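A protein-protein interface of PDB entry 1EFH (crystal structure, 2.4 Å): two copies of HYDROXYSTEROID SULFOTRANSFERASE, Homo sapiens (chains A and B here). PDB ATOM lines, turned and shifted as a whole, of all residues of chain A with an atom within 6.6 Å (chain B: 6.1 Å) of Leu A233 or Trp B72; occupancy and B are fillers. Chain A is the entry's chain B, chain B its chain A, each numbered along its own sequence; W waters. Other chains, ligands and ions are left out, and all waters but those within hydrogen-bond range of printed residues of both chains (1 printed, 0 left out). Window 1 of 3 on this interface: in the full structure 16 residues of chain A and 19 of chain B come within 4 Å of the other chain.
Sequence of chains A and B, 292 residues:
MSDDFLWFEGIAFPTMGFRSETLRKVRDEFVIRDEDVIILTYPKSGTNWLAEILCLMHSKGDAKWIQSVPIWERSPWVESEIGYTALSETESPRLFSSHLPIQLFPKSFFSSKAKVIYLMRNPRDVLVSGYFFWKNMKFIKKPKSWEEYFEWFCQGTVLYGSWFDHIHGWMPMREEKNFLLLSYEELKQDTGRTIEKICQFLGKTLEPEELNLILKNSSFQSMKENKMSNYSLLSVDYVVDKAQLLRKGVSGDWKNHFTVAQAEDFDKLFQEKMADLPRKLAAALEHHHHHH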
ATOM      1  N   MET A  16      -2.936 -23.901  22.982  1.00  0.00           N
ATOM      2  CA  MET A  16      -3.125 -23.080  21.794  1.00  0.00           C
ATOM      3  C   MET A  16      -4.052 -21.907  22.078  1.00  0.00           C
ATOM      4  O   MET A  16      -4.945 -22.006  22.914  1.00  0.00           O
ATOM      5  CB  MET A  16      -3.703 -23.909  20.649  1.00  0.00           C
ATOM      6  CG  MET A  16      -5.208 -23.892  20.590  1.00  0.00           C
ATOM      7  SD  MET A  16      -5.811 -23.300  18.998  1.00  0.00           S
ATOM      8  CE  MET A  16      -6.142 -21.583  19.342  1.00  0.00           C
ATOM      9  N   PRO A  70     -20.948 -14.858  16.059  1.00  0.00           N
ATOM     10  CA  PRO A  70     -20.568 -15.799  17.121  1.00  0.00           C
ATOM     11  C   PRO A  70     -20.291 -15.081  18.453  1.00  0.00           C
ATOM     12  O   PRO A  70     -19.734 -13.987  18.485  1.00  0.00           O
ATOM     13  CB  PRO A  70     -19.334 -16.502  16.545  1.00  0.00           C
ATOM     14  CG  PRO A  70     -18.785 -15.506  15.567  1.00  0.00           C
ATOM     15  CD  PRO A  70     -20.025 -14.950  14.916  1.00  0.00           C
ATOM     16  N   TRP A  72     -18.104 -15.508  20.860  1.00  0.00           N
ATOM     17  CA  TRP A  72     -16.723 -15.145  21.165  1.00  0.00           C
ATOM     18  C   TRP A  72     -16.284 -13.873  20.439  1.00  0.00           C
ATOM     19  O   TRP A  72     -15.200 -13.347  20.683  1.00  0.00           O
ATOM     20  CB  TRP A  72     -15.770 -16.303  20.836  1.00  0.00           C
ATOM     21  CG  TRP A  72     -16.074 -17.016  19.548  1.00  0.00           C
ATOM     22  CD1 TRP A  72     -16.752 -18.199  19.397  1.00  0.00           C
ATOM     23  CD2 TRP A  72     -15.728 -16.582  18.232  1.00  0.00           C
ATOM     24  NE1 TRP A  72     -16.846 -18.524  18.064  1.00  0.00           N
ATOM     25  CE2 TRP A  72     -16.226 -17.549  17.328  1.00  0.00           C
ATOM     26  CE3 TRP A  72     -15.046 -15.468  17.726  1.00  0.00           C
ATOM     27  CZ2 TRP A  72     -16.065 -17.432  15.947  1.00  0.00           C
ATOM     28  CZ3 TRP A  72     -14.884 -15.350  16.352  1.00  0.00           C
ATOM     29  CH2 TRP A  72     -15.393 -16.329  15.478  1.00  0.00           C
ATOM     30  N   TRP A  77     -12.554 -12.985  24.599  1.00  0.00           N
ATOM     31  CA  TRP A  77     -11.797 -13.477  25.740  1.00  0.00           C
ATOM     32  C   TRP A  77     -10.505 -12.642  25.717  1.00  0.00           C
ATOM     33  O   TRP A  77      -9.590 -12.930  24.950  1.00  0.00           O
ATOM     34  CB  TRP A  77     -11.509 -14.957  25.479  1.00  0.00           C
ATOM     35  CG  TRP A  77     -11.014 -15.761  26.620  1.00  0.00           C
ATOM     36  CD1 TRP A  77     -10.443 -15.302  27.763  1.00  0.00           C
ATOM     37  CD2 TRP A  77     -10.948 -17.192  26.681  1.00  0.00           C
ATOM     38  NE1 TRP A  77     -10.015 -16.359  28.537  1.00  0.00           N
ATOM     39  CE2 TRP A  77     -10.314 -17.531  27.894  1.00  0.00           C
ATOM     40  CE3 TRP A  77     -11.362 -18.221  25.823  1.00  0.00           C
ATOM     41  CZ2 TRP A  77     -10.079 -18.854  28.275  1.00  0.00           C
ATOM     42  CZ3 TRP A  77     -11.128 -19.545  26.201  1.00  0.00           C
ATOM     43  CH2 TRP A  77     -10.492 -19.844  27.419  1.00  0.00           C
ATOM     44  N   ILE A  82      -6.632 -14.104  19.977  1.00  0.00           N
ATOM     45  CA  ILE A  82      -7.700 -13.522  19.186  1.00  0.00           C
ATOM     46  C   ILE A  82      -8.361 -12.344  19.902  1.00  0.00           C
ATOM     47  O   ILE A  82      -8.496 -11.248  19.339  1.00  0.00           O
ATOM     48  CB  ILE A  82      -8.774 -14.577  18.876  1.00  0.00           C
ATOM     49  CG1 ILE A  82      -8.130 -15.794  18.207  1.00  0.00           C
ATOM     50  CG2 ILE A  82      -9.830 -13.983  17.966  1.00  0.00           C
ATOM     51  CD1 ILE A  82      -9.046 -17.005  18.114  1.00  0.00           C
ATOM     52  N   MET A 228     -24.498 -20.012  17.244  1.00  0.00           N
ATOM     53  CA  MET A 228     -23.619 -18.862  17.425  1.00  0.00           C
ATOM     54  C   MET A 228     -23.157 -18.750  18.873  1.00  0.00           C
ATOM     55  O   MET A 228     -22.082 -18.211  19.149  1.00  0.00           O
ATOM     56  CB  MET A 228     -24.336 -17.560  17.044  1.00  0.00           C
ATOM     57  CG  MET A 228     -24.538 -17.330  15.554  1.00  0.00           C
ATOM     58  SD  MET A 228     -22.996 -17.375  14.613  1.00  0.00           S
ATOM     59  CE  MET A 228     -23.174 -18.950  13.898  1.00  0.00           C
ATOM     60  N   TYR A 231     -21.290 -22.664  21.459  1.00  0.00           N
ATOM     61  CA  TYR A 231     -19.982 -23.077  20.980  1.00  0.00           C
ATOM     62  C   TYR A 231     -18.870 -22.168  21.487  1.00  0.00           C
ATOM     63  O   TYR A 231     -19.124 -21.056  21.947  1.00  0.00           O
ATOM     64  CB  TYR A 231     -19.950 -23.108  19.450  1.00  0.00           C
ATOM     65  CG  TYR A 231     -19.077 -24.222  18.929  1.00  0.00           C
ATOM     66  CD1 TYR A 231     -19.429 -25.558  19.147  1.00  0.00           C
ATOM     67  CD2 TYR A 231     -17.867 -23.950  18.294  1.00  0.00           C
ATOM     68  CE1 TYR A 231     -18.593 -26.599  18.756  1.00  0.00           C
ATOM     69  CE2 TYR A 231     -17.019 -24.986  17.896  1.00  0.00           C
ATOM     70  CZ  TYR A 231     -17.387 -26.310  18.135  1.00  0.00           C
ATOM     71  OH  TYR A 231     -16.547 -27.344  17.774  1.00  0.00           O
ATOM     72  N   SER A 232     -17.637 -22.661  21.402  1.00  0.00           N
ATOM     73  CA  SER A 232     -16.461 -21.913  21.837  1.00  0.00           C
ATOM     74  C   SER A 232     -15.274 -22.229  20.928  1.00  0.00           C
ATOM     75  O   SER A 232     -15.237 -23.286  20.293  1.00  0.00           O
ATOM     76  CB  SER A 232     -16.116 -22.274  23.283  1.00  0.00           C
ATOM     77  OG  SER A 232     -15.950 -23.672  23.427  1.00  0.00           O
ATOM     78  N   LEU A 233     -14.310 -21.313  20.860  1.00  0.00           N
ATOM     79  CA  LEU A 233     -13.124 -21.511  20.030  1.00  0.00           C
ATOM     80  C   LEU A 233     -12.064 -22.365  20.726  1.00  0.00           C
ATOM     81  O   LEU A 233     -10.918 -21.944  20.903  1.00  0.00           O
ATOM     82  CB  LEU A 233     -12.516 -20.163  19.625  1.00  0.00           C
ATOM     83  CG  LEU A 233     -13.223 -19.376  18.516  1.00  0.00           C
ATOM     84  CD1 LEU A 233     -12.501 -18.056  18.274  1.00  0.00           C
ATOM     85  CD2 LEU A 233     -13.239 -20.202  17.241  1.00  0.00           C
ATOM     86  N   LEU A 234     -12.461 -23.568  21.121  1.00  0.00           N
ATOM     87  CA  LEU A 234     -11.561 -24.505  21.782  1.00  0.00           C
ATOM     88  C   LEU A 234     -11.698 -25.857  21.089  1.00  0.00           C
ATOM     89  O   LEU A 234     -12.630 -26.615  21.368  1.00  0.00           O
ATOM     90  CB  LEU A 234     -11.917 -24.627  23.268  1.00  0.00           C
ATOM     91  CG  LEU A 234     -11.636 -23.404  24.150  1.00  0.00           C
ATOM     92  CD1 LEU A 234     -12.241 -23.610  25.527  1.00  0.00           C
ATOM     93  CD2 LEU A 234     -10.133 -23.176  24.254  1.00  0.00           C
ATOM     94  N   SER A 235     -10.775 -26.145  20.175  1.00  0.00           N
ATOM     95  CA  SER A 235     -10.789 -27.400  19.426  1.00  0.00           C
ATOM     96  C   SER A 235     -10.929 -28.616  20.340  1.00  0.00           C
ATOM     97  O   SER A 235     -10.174 -28.777  21.299  1.00  0.00           O
ATOM     98  CB  SER A 235      -9.514 -27.533  18.587  1.00  0.00           C
ATOM     99  OG  SER A 235      -9.463 -26.554  17.566  1.00  0.00           O
ATOM    100  N   ASN B  48     -15.714 -25.283   0.256  1.00  0.00           N
ATOM    101  CA  ASN B  48     -16.494 -25.939   1.295  1.00  0.00           C
ATOM    102  C   ASN B  48     -17.036 -27.301   0.892  1.00  0.00           C
ATOM    103  O   ASN B  48     -17.132 -28.204   1.717  1.00  0.00           O
ATOM    104  CB  ASN B  48     -17.636 -25.029   1.727  1.00  0.00           C
ATOM    105  CG  ASN B  48     -17.143 -23.845   2.521  1.00  0.00           C
ATOM    106  OD1 ASN B  48     -16.628 -24.005   3.637  1.00  0.00           O
ATOM    107  ND2 ASN B  48     -17.273 -22.647   1.951  1.00  0.00           N
ATOM    108  N   PRO B  70     -18.557 -27.281  13.541  1.00  0.00           N
ATOM    109  CA  PRO B  70     -18.635 -26.456  12.328  1.00  0.00           C
ATOM    110  C   PRO B  70     -17.540 -26.787  11.309  1.00  0.00           C
ATOM    111  O   PRO B  70     -16.462 -27.268  11.665  1.00  0.00           O
ATOM    112  CB  PRO B  70     -18.561 -25.025  12.871  1.00  0.00           C
ATOM    113  CG  PRO B  70     -17.767 -25.177  14.129  1.00  0.00           C
ATOM    114  CD  PRO B  70     -18.305 -26.454  14.733  1.00  0.00           C
ATOM    115  N   ILE B  71     -17.829 -26.533  10.039  1.00  0.00           N
ATOM    116  CA  ILE B  71     -16.883 -26.835   8.976  1.00  0.00           C
ATOM    117  C   ILE B  71     -15.561 -26.059   9.076  1.00  0.00           C
ATOM    118  O   ILE B  71     -14.491 -26.652   8.905  1.00  0.00           O
ATOM    119  CB  ILE B  71     -17.532 -26.608   7.583  1.00  0.00           C
ATOM    120  CG1 ILE B  71     -16.727 -27.342   6.508  1.00  0.00           C
ATOM    121  CG2 ILE B  71     -17.623 -25.122   7.282  1.00  0.00           C
ATOM    122  CD1 ILE B  71     -17.390 -27.378   5.149  1.00  0.00           C
ATOM    123  N   TRP B  72     -15.619 -24.756   9.358  1.00  0.00           N
ATOM    124  CA  TRP B  72     -14.390 -23.965   9.463  1.00  0.00           C
ATOM    125  C   TRP B  72     -13.462 -24.439  10.585  1.00  0.00           C
ATOM    126  O   TRP B  72     -12.306 -24.022  10.672  1.00  0.00           O
ATOM    127  CB  TRP B  72     -14.690 -22.467   9.629  1.00  0.00           C
ATOM    128  CG  TRP B  72     -15.800 -22.156  10.571  1.00  0.00           C
ATOM    129  CD1 TRP B  72     -17.115 -21.949  10.253  1.00  0.00           C
ATOM    130  CD2 TRP B  72     -15.711 -22.050  11.994  1.00  0.00           C
ATOM    131  NE1 TRP B  72     -17.848 -21.720  11.390  1.00  0.00           N
ATOM    132  CE2 TRP B  72     -17.013 -21.777  12.475  1.00  0.00           C
ATOM    133  CE3 TRP B  72     -14.657 -22.163  12.911  1.00  0.00           C
ATOM    134  CZ2 TRP B  72     -17.292 -21.613  13.834  1.00  0.00           C
ATOM    135  CZ3 TRP B  72     -14.934 -22.001  14.268  1.00  0.00           C
ATOM    136  CH2 TRP B  72     -16.244 -21.729  14.714  1.00  0.00           C
ATOM    137  N   GLU B  73     -13.959 -25.318  11.442  1.00  0.00           N
ATOM    138  CA  GLU B  73     -13.112 -25.838  12.498  1.00  0.00           C
ATOM    139  C   GLU B  73     -12.501 -27.159  12.022  1.00  0.00           C
ATOM    140  O   GLU B  73     -11.370 -27.500  12.381  1.00  0.00           O
ATOM    141  CB  GLU B  73     -13.914 -26.046  13.791  1.00  0.00           C
ATOM    142  CG  GLU B  73     -13.157 -26.832  14.862  1.00  0.00           C
ATOM    143  CD  GLU B  73     -13.785 -26.716  16.243  1.00  0.00           C
ATOM    144  OE1 GLU B  73     -13.457 -27.557  17.116  1.00  0.00           O
ATOM    145  OE2 GLU B  73     -14.590 -25.778  16.455  1.00  0.00           O
ATOM    146  N   ARG B  74     -13.254 -27.887  11.200  1.00  0.00           N
ATOM    147  CA  ARG B  74     -12.793 -29.167  10.671  1.00  0.00           C
ATOM    148  C   ARG B  74     -11.740 -28.945   9.584  1.00  0.00           C
ATOM    149  O   ARG B  74     -10.855 -29.775   9.372  1.00  0.00           O
ATOM    150  CB  ARG B  74     -13.987 -29.967  10.126  1.00  0.00           C
ATOM    151  CG  ARG B  74     -14.943 -30.443  11.224  1.00  0.00           C
ATOM    152  CD  ARG B  74     -16.068 -31.341  10.699  1.00  0.00           C
ATOM    153  NE  ARG B  74     -17.268 -30.595  10.313  1.00  0.00           N
ATOM    154  CZ  ARG B  74     -17.699 -30.432   9.064  1.00  0.00           C
ATOM    155  NH1 ARG B  74     -17.030 -30.956   8.046  1.00  0.00           N
ATOM    156  NH2 ARG B  74     -18.814 -29.752   8.832  1.00  0.00           N
ATOM    157  N   SER B  75     -11.840 -27.810   8.907  1.00  0.00           N
ATOM    158  CA  SER B  75     -10.903 -27.452   7.855  1.00  0.00           C
ATOM    159  C   SER B  75     -10.697 -25.945   7.923  1.00  0.00           C
ATOM    160  O   SER B  75     -11.322 -25.188   7.184  1.00  0.00           O
ATOM    161  CB  SER B  75     -11.463 -27.843   6.481  1.00  0.00           C
ATOM    162  OG  SER B  75     -10.580 -27.445   5.447  1.00  0.00           O
ATOM    163  N   PRO B  76      -9.811 -25.490   8.818  1.00  0.00           N
ATOM    164  CA  PRO B  76      -9.537 -24.062   8.977  1.00  0.00           C
ATOM    165  C   PRO B  76      -9.010 -23.369   7.722  1.00  0.00           C
ATOM    166  O   PRO B  76      -8.417 -23.989   6.841  1.00  0.00           O
ATOM    167  CB  PRO B  76      -8.513 -24.025  10.119  1.00  0.00           C
ATOM    168  CG  PRO B  76      -8.816 -25.255  10.892  1.00  0.00           C
ATOM    169  CD  PRO B  76      -9.049 -26.276   9.804  1.00  0.00           C
ATOM    170  N   TRP B  77      -9.242 -22.066   7.673  1.00  0.00           N
ATOM    171  CA  TRP B  77      -8.801 -21.200   6.590  1.00  0.00           C
ATOM    172  C   TRP B  77      -7.476 -20.646   7.137  1.00  0.00           C
ATOM    173  O   TRP B  77      -7.464 -19.640   7.848  1.00  0.00           O
ATOM    174  CB  TRP B  77      -9.844 -20.101   6.437  1.00  0.00           C
ATOM    175  CG  TRP B  77      -9.699 -19.199   5.288  1.00  0.00           C
ATOM    176  CD1 TRP B  77      -8.659 -19.130   4.411  1.00  0.00           C
ATOM    177  CD2 TRP B  77     -10.627 -18.183   4.900  1.00  0.00           C
ATOM    178  NE1 TRP B  77      -8.881 -18.122   3.491  1.00  0.00           N
ATOM    179  CE2 TRP B  77     -10.083 -17.526   3.772  1.00  0.00           C
ATOM    180  CE3 TRP B  77     -11.869 -17.760   5.399  1.00  0.00           C
ATOM    181  CZ2 TRP B  77     -10.738 -16.469   3.132  1.00  0.00           C
ATOM    182  CZ3 TRP B  77     -12.526 -16.703   4.757  1.00  0.00           C
ATOM    183  CH2 TRP B  77     -11.954 -16.074   3.636  1.00  0.00           C
ATOM    184  N   ILE B  82      -8.231 -16.755  12.880  1.00  0.00           N
ATOM    185  CA  ILE B  82      -8.662 -17.950  13.585  1.00  0.00           C
ATOM    186  C   ILE B  82      -7.966 -19.214  13.091  1.00  0.00           C
ATOM    187  O   ILE B  82      -7.546 -20.055  13.895  1.00  0.00           O
ATOM    188  CB  ILE B  82     -10.191 -18.121  13.456  1.00  0.00           C
ATOM    189  CG1 ILE B  82     -10.890 -16.974  14.191  1.00  0.00           C
ATOM    190  CG2 ILE B  82     -10.633 -19.464  14.023  1.00  0.00           C
ATOM    191  CD1 ILE B  82     -12.354 -16.837  13.844  1.00  0.00           C
ATOM    192  N   MET B 228     -23.865 -26.868  10.646  1.00  0.00           N
ATOM    193  CA  MET B 228     -22.422 -26.891  10.874  1.00  0.00           C
ATOM    194  C   MET B 228     -21.578 -26.677   9.614  1.00  0.00           C
ATOM    195  O   MET B 228     -20.450 -26.178   9.691  1.00  0.00           O
ATOM    196  CB  MET B 228     -22.011 -28.217  11.522  1.00  0.00           C
ATOM    197  CG  MET B 228     -22.542 -28.430  12.929  1.00  0.00           C
ATOM    198  SD  MET B 228     -21.993 -27.169  14.101  1.00  0.00           S
ATOM    199  CE  MET B 228     -23.341 -25.999  13.975  1.00  0.00           C
ATOM    200  N   TYR B 231     -22.062 -22.887   7.181  1.00  0.00           N
ATOM    201  CA  TYR B 231     -21.616 -21.935   8.203  1.00  0.00           C
ATOM    202  C   TYR B 231     -20.278 -21.279   7.816  1.00  0.00           C
ATOM    203  O   TYR B 231     -19.242 -21.946   7.759  1.00  0.00           O
ATOM    204  CB  TYR B 231     -21.468 -22.731   9.508  1.00  0.00           C
ATOM    205  CG  TYR B 231     -21.205 -21.980  10.799  1.00  0.00           C
ATOM    206  CD1 TYR B 231     -21.141 -22.679  12.014  1.00  0.00           C
ATOM    207  CD2 TYR B 231     -21.025 -20.597  10.825  1.00  0.00           C
ATOM    208  CE1 TYR B 231     -20.908 -22.025  13.223  1.00  0.00           C
ATOM    209  CE2 TYR B 231     -20.786 -19.927  12.034  1.00  0.00           C
ATOM    210  CZ  TYR B 231     -20.731 -20.651  13.230  1.00  0.00           C
ATOM    211  OH  TYR B 231     -20.529 -20.000  14.430  1.00  0.00           O
ATOM    212  N   SER B 232     -20.310 -19.976   7.548  1.00  0.00           N
ATOM    213  CA  SER B 232     -19.110 -19.218   7.181  1.00  0.00           C
ATOM    214  C   SER B 232     -18.820 -18.153   8.238  1.00  0.00           C
ATOM    215  O   SER B 232     -19.729 -17.454   8.682  1.00  0.00           O
ATOM    216  CB  SER B 232     -19.308 -18.539   5.820  1.00  0.00           C
ATOM    217  OG  SER B 232     -18.271 -17.607   5.556  1.00  0.00           O
ATOM    218  N   LEU B 233     -17.558 -18.024   8.634  1.00  0.00           N
ATOM    219  CA  LEU B 233     -17.181 -17.041   9.650  1.00  0.00           C
ATOM    220  C   LEU B 233     -17.040 -15.613   9.132  1.00  0.00           C
ATOM    221  O   LEU B 233     -16.716 -14.699   9.896  1.00  0.00           O
ATOM    222  CB  LEU B 233     -15.887 -17.458  10.356  1.00  0.00           C
ATOM    223  CG  LEU B 233     -15.981 -18.665  11.299  1.00  0.00           C
ATOM    224  CD1 LEU B 233     -14.641 -18.863  11.984  1.00  0.00           C
ATOM    225  CD2 LEU B 233     -17.078 -18.444  12.339  1.00  0.00           C
HETATM  226  O   HOH W   1      -9.303 -26.485  14.628  1.00  0.00           O
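OH of Tyr A231 sits at hydrogen-bond distance from OE2 of Glu B73 (2.8 Å). The side-chain hydroxyl (OH) of Tyr B231 lies close to the side-chain sulfur (SD) of Met A228, 3.6 Å away.
CH2 of Trp A72 touches CD1 of Ile B82, 3.5 Å away. Trp A72 touches Leu B233 (CZ2 to CD2, 3.9 Å). CZ of Tyr A231 touches CD of Pro B70, at 3.5 Å. Leu A233 touches Trp B72. Ser A235 touches Glu B73.
Of chain B, only Trp B72 (3.9 Å) comes within 4 Å of Leu A233. Trp B72 touches one residue of chain A. Of the printed residues of chain A, Leu B233 touches Trp A72 (3.9 Å). Printed residues of chain A within 4 Å of Glu B73: Tyr A231 (2.8 Å) and Ser A235 (3.5 Å). Of the printed residues of chain B, Trp A72 touches Ile B82 (3.5 Å) and Leu B233 (3.9 Å). Pro B76 touches none of the printed residues of chain A. The nearest residue of chain A that does not touch Trp B72 is Trp A72 (4.5 Å).
Of the 11 printed residues of chain A, 5 touch a printed residue of chain B. Printed residues of chain A that touch a printed residue of chain B: Trp A72, Met A228, Tyr A231, Leu A233 and Ser A235. Hydrophobic or aromatic side chains of chain A within 4 Å of the printed part of chain B: Trp A72, Met A228, Tyr A231 and Leu A233. Along chain A the printed residues that touch a printed residue of chain B span positions 72 to 235. Of the 14 printed residues of chain B, 6 touch a printed residue of chain A. Among the printed residues, 7 pairs touch across the chains. Among the printed residues, no Asp or Glu carboxylate lies within 4 Å of a Lys or Arg side-chain nitrogen of the other chain.
Trp A72 touches Ile B82, but with the chains exchanged Ile A82 does not touch Trp B72 (8.6 Å). Trp A72 touches Leu B233, and with the chains exchanged Leu A233 touches Trp B72. Met A228 touches Tyr B231, but with the chains exchanged Tyr A231 does not touch Met B228 (5.8 Å). Tyr A231 touches Pro B70, but with the chains exchanged Pro A70 does not touch Tyr B231 (4.3 Å).
Water W1 bridges the side-chain hydroxyl of Ser A235 and the backbone carbonyl oxygen of Glu B73.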
